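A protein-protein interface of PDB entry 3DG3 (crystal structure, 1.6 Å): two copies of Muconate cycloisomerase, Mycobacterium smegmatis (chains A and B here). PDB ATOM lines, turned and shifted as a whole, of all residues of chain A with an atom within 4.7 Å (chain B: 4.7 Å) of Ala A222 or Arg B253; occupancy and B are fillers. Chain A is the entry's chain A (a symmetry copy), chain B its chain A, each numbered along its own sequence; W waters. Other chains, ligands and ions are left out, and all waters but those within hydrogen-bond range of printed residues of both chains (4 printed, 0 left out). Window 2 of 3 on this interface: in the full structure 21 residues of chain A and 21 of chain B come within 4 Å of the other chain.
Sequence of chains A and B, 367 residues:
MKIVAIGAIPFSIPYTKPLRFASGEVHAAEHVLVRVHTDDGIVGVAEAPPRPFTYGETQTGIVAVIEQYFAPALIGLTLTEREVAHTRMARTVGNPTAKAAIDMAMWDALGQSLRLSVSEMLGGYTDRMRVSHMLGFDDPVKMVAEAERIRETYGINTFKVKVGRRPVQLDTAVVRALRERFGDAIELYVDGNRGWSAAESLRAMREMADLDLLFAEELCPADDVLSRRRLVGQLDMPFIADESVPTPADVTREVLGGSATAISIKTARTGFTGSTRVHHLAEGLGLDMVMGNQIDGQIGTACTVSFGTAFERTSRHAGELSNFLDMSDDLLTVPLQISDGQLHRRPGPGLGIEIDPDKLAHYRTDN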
ATOM      1  N   GLU A 218       9.457   7.402 -24.993  1.00  0.00           N
ATOM      2  CA  GLU A 218       8.071   7.598 -24.554  1.00  0.00           C
ATOM      3  C   GLU A 218       7.033   7.345 -25.649  1.00  0.00           C
ATOM      4  O   GLU A 218       6.173   8.187 -25.903  1.00  0.00           O
ATOM      5  CB  GLU A 218       7.899   9.028 -24.025  1.00  0.00           C
ATOM      6  CG  GLU A 218       8.707   9.375 -22.778  1.00  0.00           C
ATOM      7  CD  GLU A 218       8.092   8.820 -21.503  1.00  0.00           C
ATOM      8  OE1 GLU A 218       7.020   8.193 -21.585  1.00  0.00           O
ATOM      9  OE2 GLU A 218       8.682   9.017 -20.420  1.00  0.00           O
ATOM     10  N   CYS A 220       4.459   5.348 -25.702  1.00  0.00           N
ATOM     11  CA  CYS A 220       3.125   5.283 -25.114  1.00  0.00           C
ATOM     12  C   CYS A 220       3.171   5.843 -23.692  1.00  0.00           C
ATOM     13  O   CYS A 220       4.248   6.099 -23.150  1.00  0.00           O
ATOM     14  CB  CYS A 220       2.635   3.833 -25.083  1.00  0.00           C
ATOM     15  SG  CYS A 220       3.532   2.781 -23.897  1.00  0.00           S
ATOM     16  N   PRO A 221       2.000   6.054 -23.068  1.00  0.00           N
ATOM     17  CA  PRO A 221       1.989   6.590 -21.705  1.00  0.00           C
ATOM     18  C   PRO A 221       2.621   5.644 -20.692  1.00  0.00           C
ATOM     19  O   PRO A 221       2.325   4.447 -20.684  1.00  0.00           O
ATOM     20  CB  PRO A 221       0.498   6.783 -21.414  1.00  0.00           C
ATOM     21  CG  PRO A 221      -0.109   6.940 -22.771  1.00  0.00           C
ATOM     22  CD  PRO A 221       0.629   5.914 -23.587  1.00  0.00           C
ATOM     23  N   ALA A 222       3.482   6.174 -19.831  1.00  0.00           N
ATOM     24  CA  ALA A 222       4.092   5.340 -18.807  1.00  0.00           C
ATOM     25  C   ALA A 222       2.991   4.960 -17.820  1.00  0.00           C
ATOM     26  O   ALA A 222       3.102   3.960 -17.119  1.00  0.00           O
ATOM     27  CB  ALA A 222       5.204   6.101 -18.082  1.00  0.00           C
ATOM     28  N   ASP A 223       1.922   5.756 -17.775  1.00  0.00           N
ATOM     29  CA  ASP A 223       0.821   5.475 -16.861  1.00  0.00           C
ATOM     30  C   ASP A 223      -0.082   4.326 -17.332  1.00  0.00           C
ATOM     31  O   ASP A 223      -0.988   3.905 -16.611  1.00  0.00           O
ATOM     32  CB  ASP A 223       0.022   6.754 -16.576  1.00  0.00           C
ATOM     33  CG  ASP A 223       0.746   7.696 -15.603  1.00  0.00           C
ATOM     34  OD1 ASP A 223       1.859   7.365 -15.134  1.00  0.00           O
ATOM     35  OD2 ASP A 223       0.193   8.772 -15.294  1.00  0.00           O
ATOM     36  N   ASP A 224       0.148   3.825 -18.546  1.00  0.00           N
ATOM     37  CA  ASP A 224      -0.584   2.635 -19.011  1.00  0.00           C
ATOM     38  C   ASP A 224       0.442   1.615 -18.520  1.00  0.00           C
ATOM     39  O   ASP A 224       1.077   0.903 -19.301  1.00  0.00           O
ATOM     40  CB  ASP A 224      -0.678   2.588 -20.542  1.00  0.00           C
ATOM     41  CG  ASP A 224      -1.768   3.491 -21.096  1.00  0.00           C
ATOM     42  OD1 ASP A 224      -2.455   4.166 -20.302  1.00  0.00           O
ATOM     43  OD2 ASP A 224      -1.939   3.518 -22.338  1.00  0.00           O
ATOM     44  N   VAL A 225       0.587   1.573 -17.198  1.00  0.00           N
ATOM     45  CA  VAL A 225       1.606   0.774 -16.530  1.00  0.00           C
ATOM     46  C   VAL A 225       1.982  -0.607 -17.046  1.00  0.00           C
ATOM     47  O   VAL A 225       3.113  -0.800 -17.498  1.00  0.00           O
ATOM     48  CB  VAL A 225       1.329   0.674 -15.008  1.00  0.00           C
ATOM     49  CG1 VAL A 225       2.508  -0.005 -14.311  1.00  0.00           C
ATOM     50  CG2 VAL A 225       1.128   2.069 -14.424  1.00  0.00           C
ATOM     51  N   ARG A 228       2.851  -0.754 -20.826  1.00  0.00           N
ATOM     52  CA  ARG A 228       4.101  -0.032 -21.044  1.00  0.00           C
ATOM     53  C   ARG A 228       5.260  -0.978 -20.734  1.00  0.00           C
ATOM     54  O   ARG A 228       6.226  -1.072 -21.495  1.00  0.00           O
ATOM     55  CB  ARG A 228       4.162   1.184 -20.114  1.00  0.00           C
ATOM     56  CG  ARG A 228       5.548   1.786 -19.914  1.00  0.00           C
ATOM     57  CD  ARG A 228       6.023   2.671 -21.063  1.00  0.00           C
ATOM     58  NE  ARG A 228       7.140   3.499 -20.599  1.00  0.00           N
ATOM     59  CZ  ARG A 228       7.269   4.800 -20.849  1.00  0.00           C
ATOM     60  NH1 ARG A 228       6.356   5.440 -21.575  1.00  0.00           N
ATOM     61  NH2 ARG A 228       8.293   5.472 -20.335  1.00  0.00           N
ATOM     62  N   ARG A 229       5.166  -1.686 -19.613  1.00  0.00           N
ATOM     63  CA  ARG A 229       6.230  -2.612 -19.247  1.00  0.00           C
ATOM     64  C   ARG A 229       6.381  -3.721 -20.276  1.00  0.00           C
ATOM     65  O   ARG A 229       7.501  -4.124 -20.605  1.00  0.00           O
ATOM     66  CB  ARG A 229       5.961  -3.219 -17.866  1.00  0.00           C
ATOM     67  CG  ARG A 229       6.005  -2.183 -16.759  1.00  0.00           C
ATOM     68  CD  ARG A 229       5.634  -2.753 -15.399  1.00  0.00           C
ATOM     69  NE  ARG A 229       5.747  -1.705 -14.387  1.00  0.00           N
ATOM     70  CZ  ARG A 229       5.692  -1.904 -13.075  1.00  0.00           C
ATOM     71  NH1 ARG A 229       5.515  -3.124 -12.582  1.00  0.00           N
ATOM     72  NH2 ARG A 229       5.851  -0.874 -12.253  1.00  0.00           N
ATOM     73  N   SER A 244       8.192  10.870 -17.816  1.00  0.00           N
ATOM     74  CA  SER A 244       7.847   9.957 -16.725  1.00  0.00           C
ATOM     75  C   SER A 244       8.940   9.795 -15.664  1.00  0.00           C
ATOM     76  O   SER A 244       8.735   9.099 -14.668  1.00  0.00           O
ATOM     77  CB  SER A 244       7.474   8.581 -17.280  1.00  0.00           C
ATOM     78  OG  SER A 244       8.554   8.013 -17.998  1.00  0.00           O
ATOM     79  N   GLU A 254      10.645   3.529 -12.259  1.00  0.00           N
ATOM     80  CA  GLU A 254      10.395   3.146 -13.642  1.00  0.00           C
ATOM     81  C   GLU A 254      11.423   2.133 -14.147  1.00  0.00           C
ATOM     82  O   GLU A 254      11.085   1.209 -14.879  1.00  0.00           O
ATOM     83  CB  GLU A 254      10.396   4.384 -14.545  1.00  0.00           C
ATOM     84  CG  GLU A 254       9.378   5.474 -14.164  1.00  0.00           C
ATOM     85  CD  GLU A 254       7.920   5.052 -14.310  1.00  0.00           C
ATOM     86  OE1 GLU A 254       7.563   4.425 -15.333  1.00  0.00           O
ATOM     87  OE2 GLU A 254       7.119   5.378 -13.404  1.00  0.00           O
ATOM     88  N   ALA B 249      -2.344   5.663 -11.480  1.00  0.00           N
ATOM     89  CA  ALA B 249      -1.086   5.083 -11.953  1.00  0.00           C
ATOM     90  C   ALA B 249      -0.096   4.945 -10.801  1.00  0.00           C
ATOM     91  O   ALA B 249       0.693   4.002 -10.758  1.00  0.00           O
ATOM     92  CB  ALA B 249      -0.483   5.938 -13.063  1.00  0.00           C
ATOM     93  N   ASP B 250      -0.121   5.892  -9.867  1.00  0.00           N
ATOM     94  CA  ASP B 250       0.778   5.810  -8.723  1.00  0.00           C
ATOM     95  C   ASP B 250       0.328   4.662  -7.826  1.00  0.00           C
ATOM     96  O   ASP B 250       1.156   3.945  -7.256  1.00  0.00           O
ATOM     97  CB  ASP B 250       0.796   7.127  -7.946  1.00  0.00           C
ATOM     98  CG  ASP B 250       1.495   8.236  -8.704  1.00  0.00           C
ATOM     99  OD1 ASP B 250       2.684   8.053  -9.063  1.00  0.00           O
ATOM    100  OD2 ASP B 250       0.864   9.289  -8.944  1.00  0.00           O
ATOM    101  N   VAL B 251      -0.985   4.485  -7.699  1.00  0.00           N
ATOM    102  CA  VAL B 251      -1.517   3.388  -6.898  1.00  0.00           C
ATOM    103  C   VAL B 251      -0.961   2.076  -7.461  1.00  0.00           C
ATOM    104  O   VAL B 251      -0.431   1.242  -6.727  1.00  0.00           O
ATOM    105  CB  VAL B 251      -3.068   3.350  -6.955  1.00  0.00           C
ATOM    106  CG1 VAL B 251      -3.589   2.057  -6.338  1.00  0.00           C
ATOM    107  CG2 VAL B 251      -3.647   4.551  -6.215  1.00  0.00           C
ATOM    108  N   THR B 252      -1.066   1.903  -8.773  1.00  0.00           N
ATOM    109  CA  THR B 252      -0.564   0.686  -9.398  1.00  0.00           C
ATOM    110  C   THR B 252       0.941   0.503  -9.180  1.00  0.00           C
ATOM    111  O   THR B 252       1.384  -0.566  -8.759  1.00  0.00           O
ATOM    112  CB  THR B 252      -0.882   0.679 -10.913  1.00  0.00           C
ATOM    113  OG1 THR B 252      -2.304   0.653 -11.093  1.00  0.00           O
ATOM    114  CG2 THR B 252      -0.269  -0.541 -11.592  1.00  0.00           C
ATOM    115  N   ARG B 253       1.732   1.540  -9.439  1.00  0.00           N
ATOM    116  CA  ARG B 253       3.181   1.419  -9.260  1.00  0.00           C
ATOM    117  C   ARG B 253       3.606   1.146  -7.818  1.00  0.00           C
ATOM    118  O   ARG B 253       4.469   0.300  -7.561  1.00  0.00           O
ATOM    119  CB  ARG B 253       3.896   2.683  -9.754  1.00  0.00           C
ATOM    120  CG  ARG B 253       4.059   2.784 -11.270  1.00  0.00           C
ATOM    121  CD  ARG B 253       4.912   3.996 -11.645  1.00  0.00           C
ATOM    122  NE  ARG B 253       4.240   5.263 -11.353  1.00  0.00           N
ATOM    123  CZ  ARG B 253       3.502   5.942 -12.230  1.00  0.00           C
ATOM    124  NH1 ARG B 253       3.343   5.490 -13.466  1.00  0.00           N
ATOM    125  NH2 ARG B 253       2.898   7.065 -11.863  1.00  0.00           N
ATOM    126  N   GLU B 254       3.006   1.860  -6.870  1.00  0.00           N
ATOM    127  CA  GLU B 254       3.387   1.681  -5.476  1.00  0.00           C
ATOM    128  C   GLU B 254       2.908   0.339  -4.922  1.00  0.00           C
ATOM    129  O   GLU B 254       3.612  -0.312  -4.158  1.00  0.00           O
ATOM    130  CB  GLU B 254       2.831   2.825  -4.622  1.00  0.00           C
ATOM    131  CG  GLU B 254       3.266   4.237  -5.054  1.00  0.00           C
ATOM    132  CD  GLU B 254       4.759   4.508  -4.904  1.00  0.00           C
ATOM    133  OE1 GLU B 254       5.347   4.144  -3.861  1.00  0.00           O
ATOM    134  OE2 GLU B 254       5.342   5.119  -5.830  1.00  0.00           O
ATOM    135  N   VAL B 255       1.709  -0.078  -5.313  1.00  0.00           N
ATOM    136  CA  VAL B 255       1.183  -1.345  -4.823  1.00  0.00           C
ATOM    137  C   VAL B 255       1.932  -2.533  -5.419  1.00  0.00           C
ATOM    138  O   VAL B 255       2.363  -3.426  -4.692  1.00  0.00           O
ATOM    139  CB  VAL B 255      -0.326  -1.463  -5.123  1.00  0.00           C
ATOM    140  CG1 VAL B 255      -0.803  -2.885  -4.864  1.00  0.00           C
ATOM    141  CG2 VAL B 255      -1.094  -0.481  -4.246  1.00  0.00           C
ATOM    142  N   LEU B 256       2.110  -2.546  -6.736  1.00  0.00           N
ATOM    143  CA  LEU B 256       2.818  -3.666  -7.343  1.00  0.00           C
ATOM    144  C   LEU B 256       4.296  -3.671  -6.960  1.00  0.00           C
ATOM    145  O   LEU B 256       4.926  -4.730  -6.929  1.00  0.00           O
ATOM    146  CB  LEU B 256       2.651  -3.648  -8.865  1.00  0.00           C
ATOM    147  CG  LEU B 256       1.201  -3.785  -9.344  1.00  0.00           C
ATOM    148  CD1 LEU B 256       1.185  -3.866 -10.867  1.00  0.00           C
ATOM    149  CD2 LEU B 256       0.554  -5.033  -8.736  1.00  0.00           C
ATOM    150  N   GLY B 257       4.838  -2.493  -6.655  1.00  0.00           N
ATOM    151  CA  GLY B 257       6.234  -2.390  -6.262  1.00  0.00           C
ATOM    152  C   GLY B 257       6.469  -2.753  -4.804  1.00  0.00           C
ATOM    153  O   GLY B 257       7.608  -2.974  -4.386  1.00  0.00           O
HETATM  154  O   HOH W   1       4.956   3.477 -15.151  1.00  0.00           O
HETATM  155  O   HOH W   2       6.283  -3.565  -9.884  1.00  0.00           O
HETATM  156  O   HOH W   3       0.613   9.296 -12.650  1.00  0.00           O
HETATM  157  O   HOH W   4       6.176  -0.801  -9.438  1.00  0.00           O
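Ala A222 touches just one residue of chain B: Arg B253.
Arg B253 touches just these residues of chain A: Ala A222, Asp A223 and Glu A254.
Of the printed residues of chain B, Asp A223 touches Ala B249 and Arg B253.
Printed residues of chain B within 4 Å of Val A225: Thr B252 (3.9 Å).
Printed residues of chain B within 4 Å of Glu A254: Arg B253 (3.1 Å).
Of the printed residues of chain A, Ala B249 touches Asp A223 (3.3 Å).
Of the printed residues of chain A, Thr B252 touches Val A225 (3.9 Å).
Glu B254 touches none of the printed residues of chain A.
The nearest printed residue of chain A that does not touch Arg B253 is Val A225 (4.2 Å).
The guanidinium group (NH2) of Arg B253 lies within salt-bridge range of the side-chain carboxylate (OD1) of Asp B250, at 3.0 Å.
Water W3 bridges OD2 of Asp A223 (2.7 Å) and NH2 of Arg B253 (3.3 Å).
Water W1 lies within hydrogen-bond range of O of Ala A222, OE1 of Glu A254 and NH1 of Arg B253.
Water W4 lies within hydrogen-bond range of the backbone carbonyl oxygen of Arg B253 (2.8 Å) and the guanidinium group of Arg A229 (2.8 Å).
Water W2 lies within hydrogen-bond range of NH1 of Arg A229 (2.8 Å) and O of Leu B256 (3.5 Å).
The side-chain carboxylate (OE2) of Glu A254 lies within salt-bridge range of the guanidinium group (NE) of Arg B253, at 3.5 Å.
The side-chain carboxylate (OD1) of Asp A223 is in salt-bridge range of the guanidinium group (NH1) of Arg B253 (2.9 Å).
Among the printed residues, merely in contact across the chains: Ala A222 with Arg B253 (3.97 Å), Asp A223 with Ala B249 (3.3 Å) and Val A225 with Thr B252 (3.9 Å).
Hydrophobic or aromatic side chains of chain B that line the printed part of chain A: Ala B249.
Of the 11 printed residues of chain A, 4 touch a printed residue of chain B.
Along chain A the printed residues that touch a printed residue of chain B span positions 222 to 254.
Among the printed residues, 5 pairs touch across the chains.
Position printed for both chains: 254.
Of the 5 pairs that touch across the chains among the printed residues, none has its exchanged pair printed and touching as well.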
